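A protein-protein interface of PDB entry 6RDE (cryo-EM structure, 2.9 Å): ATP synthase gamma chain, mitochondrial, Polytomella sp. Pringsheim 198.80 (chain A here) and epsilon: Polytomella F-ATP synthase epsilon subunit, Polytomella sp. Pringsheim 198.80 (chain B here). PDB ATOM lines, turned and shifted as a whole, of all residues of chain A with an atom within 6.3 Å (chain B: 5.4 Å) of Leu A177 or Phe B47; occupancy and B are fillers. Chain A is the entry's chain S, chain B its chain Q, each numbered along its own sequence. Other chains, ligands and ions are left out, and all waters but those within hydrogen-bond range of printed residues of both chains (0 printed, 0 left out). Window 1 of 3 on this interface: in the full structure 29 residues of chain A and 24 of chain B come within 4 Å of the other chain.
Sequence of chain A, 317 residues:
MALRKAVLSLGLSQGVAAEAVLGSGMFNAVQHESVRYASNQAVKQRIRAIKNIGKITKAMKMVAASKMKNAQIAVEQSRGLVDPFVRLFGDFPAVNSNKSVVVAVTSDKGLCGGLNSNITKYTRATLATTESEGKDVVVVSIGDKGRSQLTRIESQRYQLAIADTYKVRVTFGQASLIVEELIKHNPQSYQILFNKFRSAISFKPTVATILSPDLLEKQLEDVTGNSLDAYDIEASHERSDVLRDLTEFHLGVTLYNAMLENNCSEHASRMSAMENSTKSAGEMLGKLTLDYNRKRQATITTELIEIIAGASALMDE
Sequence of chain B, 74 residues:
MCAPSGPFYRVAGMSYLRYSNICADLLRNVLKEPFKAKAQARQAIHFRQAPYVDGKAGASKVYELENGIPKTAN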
ATOM      1  N   ILE A 162       5.270  14.265  14.455  1.00  0.00           N
ATOM      2  CA  ILE A 162       4.159  13.505  15.012  1.00  0.00           C
ATOM      3  C   ILE A 162       4.536  13.118  16.432  1.00  0.00           C
ATOM      4  O   ILE A 162       5.669  12.701  16.687  1.00  0.00           O
ATOM      5  CB  ILE A 162       3.824  12.267  14.157  1.00  0.00           C
ATOM      6  CG1 ILE A 162       3.257  12.672  12.797  1.00  0.00           C
ATOM      7  CG2 ILE A 162       2.804  11.385  14.832  1.00  0.00           C
ATOM      8  CD1 ILE A 162       4.251  12.660  11.697  1.00  0.00           C
ATOM      9  N   ALA A 163       3.615  13.307  17.367  1.00  0.00           N
ATOM     10  CA  ALA A 163       3.849  12.914  18.738  1.00  0.00           C
ATOM     11  C   ALA A 163       2.530  12.498  19.355  1.00  0.00           C
ATOM     12  O   ALA A 163       1.479  12.566  18.716  1.00  0.00           O
ATOM     13  CB  ALA A 163       4.507  14.041  19.529  1.00  0.00           C
ATOM     14  N   ASP A 164       2.612  12.055  20.612  1.00  0.00           N
ATOM     15  CA  ASP A 164       1.500  11.480  21.377  1.00  0.00           C
ATOM     16  C   ASP A 164       0.872  10.292  20.655  1.00  0.00           C
ATOM     17  O   ASP A 164      -0.329  10.048  20.748  1.00  0.00           O
ATOM     18  CB  ASP A 164       0.446  12.533  21.737  1.00  0.00           C
ATOM     19  CG  ASP A 164       0.956  13.547  22.748  1.00  0.00           C
ATOM     20  OD1 ASP A 164       0.469  14.695  22.736  1.00  0.00           O
ATOM     21  OD2 ASP A 164       1.854  13.200  23.546  1.00  0.00           O
ATOM     22  N   THR A 165       1.707   9.534  19.949  1.00  0.00           N
ATOM     23  CA  THR A 165       1.254   8.358  19.220  1.00  0.00           C
ATOM     24  C   THR A 165       0.925   7.208  20.162  1.00  0.00           C
ATOM     25  O   THR A 165      -0.140   6.592  20.049  1.00  0.00           O
ATOM     26  CB  THR A 165       2.329   7.942  18.220  1.00  0.00           C
ATOM     27  OG1 THR A 165       2.455   8.945  17.211  1.00  0.00           O
ATOM     28  CG2 THR A 165       1.996   6.630  17.576  1.00  0.00           C
ATOM     29  N   PHE A 172      -3.777   0.730  13.066  1.00  0.00           N
ATOM     30  CA  PHE A 172      -3.430   0.878  11.662  1.00  0.00           C
ATOM     31  C   PHE A 172      -4.061   2.119  11.057  1.00  0.00           C
ATOM     32  O   PHE A 172      -3.477   2.721  10.151  1.00  0.00           O
ATOM     33  CB  PHE A 172      -3.848  -0.351  10.861  1.00  0.00           C
ATOM     34  CG  PHE A 172      -3.334  -0.343   9.459  1.00  0.00           C
ATOM     35  CD1 PHE A 172      -4.144   0.043   8.411  1.00  0.00           C
ATOM     36  CD2 PHE A 172      -2.036  -0.707   9.191  1.00  0.00           C
ATOM     37  CE1 PHE A 172      -3.665   0.068   7.135  1.00  0.00           C
ATOM     38  CE2 PHE A 172      -1.558  -0.691   7.910  1.00  0.00           C
ATOM     39  CZ  PHE A 172      -2.375  -0.303   6.884  1.00  0.00           C
ATOM     40  N   GLY A 173      -5.251   2.501  11.518  1.00  0.00           N
ATOM     41  CA  GLY A 173      -5.856   3.733  11.048  1.00  0.00           C
ATOM     42  C   GLY A 173      -5.083   4.963  11.467  1.00  0.00           C
ATOM     43  O   GLY A 173      -5.096   5.977  10.766  1.00  0.00           O
ATOM     44  N   GLN A 174      -4.397   4.894  12.604  1.00  0.00           N
ATOM     45  CA  GLN A 174      -3.556   6.004  13.021  1.00  0.00           C
ATOM     46  C   GLN A 174      -2.302   6.079  12.172  1.00  0.00           C
ATOM     47  O   GLN A 174      -1.898   7.164  11.746  1.00  0.00           O
ATOM     48  CB  GLN A 174      -3.204   5.859  14.495  1.00  0.00           C
ATOM     49  CG  GLN A 174      -2.164   6.816  14.990  1.00  0.00           C
ATOM     50  CD  GLN A 174      -1.577   6.356  16.285  1.00  0.00           C
ATOM     51  OE1 GLN A 174      -1.404   5.167  16.499  1.00  0.00           O
ATOM     52  NE2 GLN A 174      -1.296   7.288  17.172  1.00  0.00           N
ATOM     53  N   ALA A 175      -1.697   4.928  11.881  1.00  0.00           N
ATOM     54  CA  ALA A 175      -0.522   4.872  11.028  1.00  0.00           C
ATOM     55  C   ALA A 175      -0.835   5.217   9.587  1.00  0.00           C
ATOM     56  O   ALA A 175       0.076   5.573   8.838  1.00  0.00           O
ATOM     57  CB  ALA A 175       0.092   3.484  11.084  1.00  0.00           C
ATOM     58  N   SER A 176      -2.099   5.107   9.185  1.00  0.00           N
ATOM     59  CA  SER A 176      -2.487   5.453   7.829  1.00  0.00           C
ATOM     60  C   SER A 176      -2.495   6.960   7.619  1.00  0.00           C
ATOM     61  O   SER A 176      -2.078   7.444   6.564  1.00  0.00           O
ATOM     62  CB  SER A 176      -3.857   4.870   7.537  1.00  0.00           C
ATOM     63  OG  SER A 176      -3.837   3.468   7.689  1.00  0.00           O
ATOM     64  N   LEU A 177      -2.969   7.718   8.609  1.00  0.00           N
ATOM     65  CA  LEU A 177      -2.951   9.171   8.492  1.00  0.00           C
ATOM     66  C   LEU A 177      -1.542   9.730   8.601  1.00  0.00           C
ATOM     67  O   LEU A 177      -1.246  10.773   8.010  1.00  0.00           O
ATOM     68  CB  LEU A 177      -3.846   9.794   9.550  1.00  0.00           C
ATOM     69  CG  LEU A 177      -5.327   9.547   9.313  1.00  0.00           C
ATOM     70  CD1 LEU A 177      -6.142   9.915  10.535  1.00  0.00           C
ATOM     71  CD2 LEU A 177      -5.762  10.349   8.119  1.00  0.00           C
ATOM     72  N   ILE A 178      -0.668   9.068   9.360  1.00  0.00           N
ATOM     73  CA  ILE A 178       0.743   9.426   9.338  1.00  0.00           C
ATOM     74  C   ILE A 178       1.344   9.076   7.989  1.00  0.00           C
ATOM     75  O   ILE A 178       2.214   9.794   7.483  1.00  0.00           O
ATOM     76  CB  ILE A 178       1.487   8.733  10.494  1.00  0.00           C
ATOM     77  CG1 ILE A 178       0.781   9.005  11.815  1.00  0.00           C
ATOM     78  CG2 ILE A 178       2.907   9.221  10.602  1.00  0.00           C
ATOM     79  CD1 ILE A 178       1.316   8.196  12.953  1.00  0.00           C
ATOM     80  N   VAL A 179       0.868   7.997   7.364  1.00  0.00           N
ATOM     81  CA  VAL A 179       1.335   7.653   6.028  1.00  0.00           C
ATOM     82  C   VAL A 179       0.870   8.658   4.994  1.00  0.00           C
ATOM     83  O   VAL A 179       1.652   9.026   4.118  1.00  0.00           O
ATOM     84  CB  VAL A 179       0.859   6.260   5.637  1.00  0.00           C
ATOM     85  N   GLU A 180      -0.374   9.138   5.110  1.00  0.00           N
ATOM     86  CA  GLU A 180      -0.950  10.031   4.105  1.00  0.00           C
ATOM     87  C   GLU A 180      -0.225  11.365   4.046  1.00  0.00           C
ATOM     88  O   GLU A 180      -0.060  11.937   2.965  1.00  0.00           O
ATOM     89  CB  GLU A 180      -2.424  10.268   4.402  1.00  0.00           C
ATOM     90  CG  GLU A 180      -3.322   9.140   3.996  1.00  0.00           C
ATOM     91  CD  GLU A 180      -4.768   9.459   4.254  1.00  0.00           C
ATOM     92  OE1 GLU A 180      -5.164  10.619   4.032  1.00  0.00           O
ATOM     93  OE2 GLU A 180      -5.506   8.557   4.698  1.00  0.00           O
ATOM     94  N   GLU A 181       0.222  11.872   5.193  1.00  0.00           N
ATOM     95  CA  GLU A 181       0.953  13.127   5.199  1.00  0.00           C
ATOM     96  C   GLU A 181       2.369  12.948   4.671  1.00  0.00           C
ATOM     97  O   GLU A 181       2.988  13.918   4.226  1.00  0.00           O
ATOM     98  CB  GLU A 181       0.938  13.714   6.609  1.00  0.00           C
ATOM     99  CG  GLU A 181       1.458  15.140   6.732  1.00  0.00           C
ATOM    100  CD  GLU A 181       0.595  16.158   6.016  1.00  0.00           C
ATOM    101  OE1 GLU A 181      -0.624  15.931   5.877  1.00  0.00           O
ATOM    102  OE2 GLU A 181       1.141  17.197   5.597  1.00  0.00           O
ATOM    103  N   LEU A 182       2.886  11.723   4.658  1.00  0.00           N
ATOM    104  CA  LEU A 182       4.099  11.477   3.892  1.00  0.00           C
ATOM    105  C   LEU A 182       3.823  11.405   2.396  1.00  0.00           C
ATOM    106  O   LEU A 182       4.765  11.467   1.607  1.00  0.00           O
ATOM    107  CB  LEU A 182       4.780  10.191   4.357  1.00  0.00           C
ATOM    108  CG  LEU A 182       5.078  10.026   5.846  1.00  0.00           C
ATOM    109  CD1 LEU A 182       5.896   8.778   6.075  1.00  0.00           C
ATOM    110  CD2 LEU A 182       5.795  11.238   6.394  1.00  0.00           C
ATOM    111  N   ARG B  18      -7.023   5.766   2.965  1.00  0.00           N
ATOM    112  CA  ARG B  18      -8.270   6.308   3.470  1.00  0.00           C
ATOM    113  C   ARG B  18      -9.462   5.517   2.974  1.00  0.00           C
ATOM    114  O   ARG B  18     -10.459   5.404   3.689  1.00  0.00           O
ATOM    115  CB  ARG B  18      -8.414   7.768   3.082  1.00  0.00           C
ATOM    116  CG  ARG B  18      -9.250   8.517   4.063  1.00  0.00           C
ATOM    117  CD  ARG B  18      -9.215   9.978   3.769  1.00  0.00           C
ATOM    118  NE  ARG B  18      -7.988  10.618   4.214  1.00  0.00           N
ATOM    119  CZ  ARG B  18      -7.964  11.625   5.072  1.00  0.00           C
ATOM    120  NH1 ARG B  18      -9.101  12.088   5.569  1.00  0.00           N
ATOM    121  NH2 ARG B  18      -6.812  12.169   5.425  1.00  0.00           N
ATOM    122  N   ILE B  45      -8.146   6.574  16.964  1.00  0.00           N
ATOM    123  CA  ILE B  45      -6.987   7.255  16.402  1.00  0.00           C
ATOM    124  C   ILE B  45      -6.684   8.450  17.283  1.00  0.00           C
ATOM    125  O   ILE B  45      -7.477   9.398  17.339  1.00  0.00           O
ATOM    126  CB  ILE B  45      -7.236   7.710  14.961  1.00  0.00           C
ATOM    127  CG1 ILE B  45      -7.558   6.516  14.076  1.00  0.00           C
ATOM    128  CG2 ILE B  45      -6.046   8.499  14.436  1.00  0.00           C
ATOM    129  CD1 ILE B  45      -8.083   6.914  12.758  1.00  0.00           C
ATOM    130  N   HIS B  46      -5.540   8.414  17.965  1.00  0.00           N
ATOM    131  CA  HIS B  46      -5.141   9.506  18.851  1.00  0.00           C
ATOM    132  C   HIS B  46      -3.668   9.806  18.628  1.00  0.00           C
ATOM    133  O   HIS B  46      -2.806   9.066  19.104  1.00  0.00           O
ATOM    134  CB  HIS B  46      -5.402   9.175  20.310  1.00  0.00           C
ATOM    135  CG  HIS B  46      -6.841   8.953  20.631  1.00  0.00           C
ATOM    136  ND1 HIS B  46      -7.461   7.735  20.466  1.00  0.00           N
ATOM    137  CD2 HIS B  46      -7.787   9.796  21.105  1.00  0.00           C
ATOM    138  CE1 HIS B  46      -8.727   7.837  20.825  1.00  0.00           C
ATOM    139  NE2 HIS B  46      -8.951   9.077  21.217  1.00  0.00           N
ATOM    140  N   PHE B  47      -3.391  10.898  17.930  1.00  0.00           N
ATOM    141  CA  PHE B  47      -2.043  11.429  17.796  1.00  0.00           C
ATOM    142  C   PHE B  47      -2.159  12.902  17.441  1.00  0.00           C
ATOM    143  O   PHE B  47      -3.258  13.441  17.301  1.00  0.00           O
ATOM    144  CB  PHE B  47      -1.220  10.650  16.765  1.00  0.00           C
ATOM    145  CG  PHE B  47      -1.593  10.915  15.339  1.00  0.00           C
ATOM    146  CD1 PHE B  47      -2.762  10.411  14.806  1.00  0.00           C
ATOM    147  CD2 PHE B  47      -0.746  11.636  14.519  1.00  0.00           C
ATOM    148  CE1 PHE B  47      -3.088  10.646  13.498  1.00  0.00           C
ATOM    149  CE2 PHE B  47      -1.063  11.870  13.208  1.00  0.00           C
ATOM    150  CZ  PHE B  47      -2.232  11.380  12.698  1.00  0.00           C
ATOM    151  N   ARG B  48      -1.017  13.555  17.305  1.00  0.00           N
ATOM    152  CA  ARG B  48      -0.994  14.950  16.912  1.00  0.00           C
ATOM    153  C   ARG B  48       0.164  15.174  15.960  1.00  0.00           C
ATOM    154  O   ARG B  48       1.266  14.660  16.156  1.00  0.00           O
ATOM    155  CB  ARG B  48      -0.901  15.890  18.130  1.00  0.00           C
ATOM    156  CG  ARG B  48       0.314  15.692  19.033  1.00  0.00           C
ATOM    157  CD  ARG B  48       0.414  16.747  20.114  1.00  0.00           C
ATOM    158  NE  ARG B  48       1.517  16.476  21.031  1.00  0.00           N
ATOM    159  CZ  ARG B  48       2.778  16.846  20.826  1.00  0.00           C
ATOM    160  NH1 ARG B  48       3.704  16.555  21.726  1.00  0.00           N
ATOM    161  NH2 ARG B  48       3.120  17.498  19.723  1.00  0.00           N
ATOM    162  N   GLN B  49      -0.106  15.919  14.899  1.00  0.00           N
ATOM    163  CA  GLN B  49       0.922  16.263  13.937  1.00  0.00           C
ATOM    164  C   GLN B  49       1.112  17.765  13.954  1.00  0.00           C
ATOM    165  O   GLN B  49       0.209  18.526  14.301  1.00  0.00           O
ATOM    166  CB  GLN B  49       0.577  15.781  12.526  1.00  0.00           C
ATOM    167  CG  GLN B  49      -0.766  16.249  12.028  1.00  0.00           C
ATOM    168  CD  GLN B  49      -1.051  15.798  10.620  1.00  0.00           C
ATOM    169  OE1 GLN B  49      -0.177  15.272   9.935  1.00  0.00           O
ATOM    170  NE2 GLN B  49      -2.282  15.996  10.177  1.00  0.00           N
ATOM    171  N   LYS B  61      -2.067  19.893  15.010  1.00  0.00           N
ATOM    172  CA  LYS B  61      -3.374  19.368  14.639  1.00  0.00           C
ATOM    173  C   LYS B  61      -3.625  18.036  15.325  1.00  0.00           C
ATOM    174  O   LYS B  61      -3.077  17.006  14.925  1.00  0.00           O
ATOM    175  CB  LYS B  61      -3.482  19.207  13.122  1.00  0.00           C
ATOM    176  CG  LYS B  61      -4.915  19.133  12.612  1.00  0.00           C
ATOM    177  CD  LYS B  61      -5.024  18.308  11.344  1.00  0.00           C
ATOM    178  CE  LYS B  61      -4.180  18.900  10.226  1.00  0.00           C
ATOM    179  NZ  LYS B  61      -4.401  18.218   8.920  1.00  0.00           N
ATOM    180  N   VAL B  62      -4.474  18.052  16.334  1.00  0.00           N
ATOM    181  CA  VAL B  62      -4.679  16.908  17.208  1.00  0.00           C
ATOM    182  C   VAL B  62      -5.762  16.017  16.622  1.00  0.00           C
ATOM    183  O   VAL B  62      -6.767  16.502  16.092  1.00  0.00           O
ATOM    184  CB  VAL B  62      -5.044  17.403  18.618  1.00  0.00           C
ATOM    185  CG1 VAL B  62      -5.155  16.257  19.617  1.00  0.00           C
ATOM    186  CG2 VAL B  62      -4.025  18.424  19.080  1.00  0.00           C
ATOM    187  N   TYR B  63      -5.555  14.708  16.695  1.00  0.00           N
ATOM    188  CA  TYR B  63      -6.532  13.725  16.253  1.00  0.00           C
ATOM    189  C   TYR B  63      -7.081  12.996  17.466  1.00  0.00           C
ATOM    190  O   TYR B  63      -6.313  12.517  18.300  1.00  0.00           O
ATOM    191  CB  TYR B  63      -5.897  12.727  15.290  1.00  0.00           C
ATOM    192  CG  TYR B  63      -5.635  13.279  13.916  1.00  0.00           C
ATOM    193  CD1 TYR B  63      -4.478  13.996  13.646  1.00  0.00           C
ATOM    194  CD2 TYR B  63      -6.541  13.081  12.890  1.00  0.00           C
ATOM    195  CE1 TYR B  63      -4.232  14.499  12.389  1.00  0.00           C
ATOM    196  CE2 TYR B  63      -6.303  13.580  11.632  1.00  0.00           C
ATOM    197  CZ  TYR B  63      -5.149  14.288  11.386  1.00  0.00           C
ATOM    198  OH  TYR B  63      -4.915  14.783  10.128  1.00  0.00           O
ATOM    199  N   GLU B  64      -8.410  12.932  17.584  1.00  0.00           N
ATOM    200  CA  GLU B  64      -9.037  12.297  18.741  1.00  0.00           C
ATOM    201  C   GLU B  64     -10.163  11.343  18.348  1.00  0.00           C
ATOM    202  O   GLU B  64     -10.993  11.004  19.194  1.00  0.00           O
ATOM    203  CB  GLU B  64      -9.568  13.339  19.741  1.00  0.00           C
ATOM    204  CG  GLU B  64      -8.641  14.530  20.045  1.00  0.00           C
ATOM    205  CD  GLU B  64      -9.198  15.487  21.079  1.00  0.00           C
ATOM    206  OE1 GLU B  64      -9.720  16.553  20.689  1.00  0.00           O
ATOM    207  OE2 GLU B  64      -9.100  15.174  22.285  1.00  0.00           O
ATOM    208  N   ILE B  69     -11.373   6.364  10.912  1.00  0.00           N
ATOM    209  CA  ILE B  69     -10.680   7.400  10.138  1.00  0.00           C
ATOM    210  C   ILE B  69     -11.677   8.502   9.788  1.00  0.00           C
ATOM    211  O   ILE B  69     -12.897   8.257   9.834  1.00  0.00           O
ATOM    212  CB  ILE B  69     -10.043   6.770   8.885  1.00  0.00           C
ATOM    213  CG1 ILE B  69      -8.676   7.379   8.578  1.00  0.00           C
ATOM    214  CG2 ILE B  69     -10.930   6.902   7.651  1.00  0.00           C
ATOM    215  CD1 ILE B  69      -7.837   6.530   7.673  1.00  0.00           C
ATOM    216  N   PRO B  70     -11.241   9.738   9.542  1.00  0.00           N
ATOM    217  CA  PRO B  70     -12.177  10.761   9.056  1.00  0.00           C
ATOM    218  C   PRO B  70     -12.742  10.420   7.684  1.00  0.00           C
ATOM    219  O   PRO B  70     -12.021  10.399   6.684  1.00  0.00           O
ATOM    220  CB  PRO B  70     -11.317  12.027   9.000  1.00  0.00           C
ATOM    221  CG  PRO B  70     -10.296  11.826  10.017  1.00  0.00           C
ATOM    222  CD  PRO B  70     -10.018  10.352  10.086  1.00  0.00           C
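The guanidinium group (NH2) of Arg B18 lies within salt-bridge range of the side-chain carboxylate (OE1) of Glu A180 (2.7 Å). The side-chain amide nitrogen (NE2) of Gln A174 sits at hydrogen-bond distance from the backbone carbonyl oxygen (O) of His B46 (3.0 Å). O of Arg B48 lies within hydrogen-bond range of N of Ala A163 (3.0 Å). NE of Arg B48 is in salt-bridge range of OD1 of Asp A164, at 2.7 Å. The backbone carbonyl oxygen (O) of His B46 sits close to the backbone carbonyl oxygen (O) of Asp A164 (3.1 Å).
The backbone carbonyl oxygen (O) of Glu B64 lies within hydrogen-bond range of a ring nitrogen (NE2) of His B46, at 3.5 Å. The backbone NH (N) of Tyr B63 is in hydrogen-bond range of the backbone carbonyl oxygen (O) of Phe B47 (2.7 Å). The backbone NH (N) of Lys B61 sits at hydrogen-bond distance from the backbone carbonyl oxygen (O) of Gln B49. NE2 of Gln B49 is in hydrogen-bond range of OH of Tyr B63, 2.9 Å away. O of Thr A165 lies within hydrogen-bond range of NE2 of Gln A174.
Phe B47 touches just these residues of chain A: Ile A162, Ala A163, Asp A164, Gln A174, Leu A177 and Ile A178. Of the printed residues of chain A, Pro B70 touches Leu A177. Of the printed residues of chain A, His B46 touches Asp A164 (3.1 Å), Thr A165 (3.8 Å) and Gln A174 (3.0 Å). The nearest residue of chain B that does not touch Leu A177 is Ile B69 (4.1 Å).
Among the printed residues, merely in contact across the chains: Ile A162 with Arg B48 (3.3 Å), Gln A174 with Phe B47 (3.4 Å), Leu A177 with Arg B18 (3.4 Å), Ile A162 with Phe B47 (3.6 Å), Glu A181 with Gln B49 (3.6 Å), Ile A178 with Phe B47 (3.7 Å), Asp A164 with Phe B47 (3.7 Å), Gly A173 with Ile B45 (3.7 Å), Thr A165 with His B46 (3.8 Å), Gln A174 with Ile B45 (3.8 Å), Ala A163 with Phe B47 (3.8 Å), Leu A177 with Tyr B63 (3.8 Å), Leu A177 with Phe B47 (3.9 Å) and Leu A177 with Pro B70 (3.9 Å).
Of the 12 printed residues of chain B, 8 touch a printed residue of chain A. Printed residues of chain B that touch a printed residue of chain A: Arg B18, Ile B45, His B46, Phe B47, Arg B48, Gln B49, Tyr B63 and Pro B70. Hydrophobic or aromatic side chains of chain B that line the printed part of chain A: Ile B45, Phe B47, Tyr B63 and Pro B70. Hydrophobic or aromatic side chains of chain A within 4 Å of the printed part of chain B: Ile A162, Ala A163, Leu A177 and Ile A178. Among the printed residues, Asp or Glu carboxylates within 4 Å of a Lys or Arg side-chain nitrogen of the other chain: Asp A164 with Arg B48 (2.7 Å) and Glu A180 with Arg B18 (2.7 Å).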
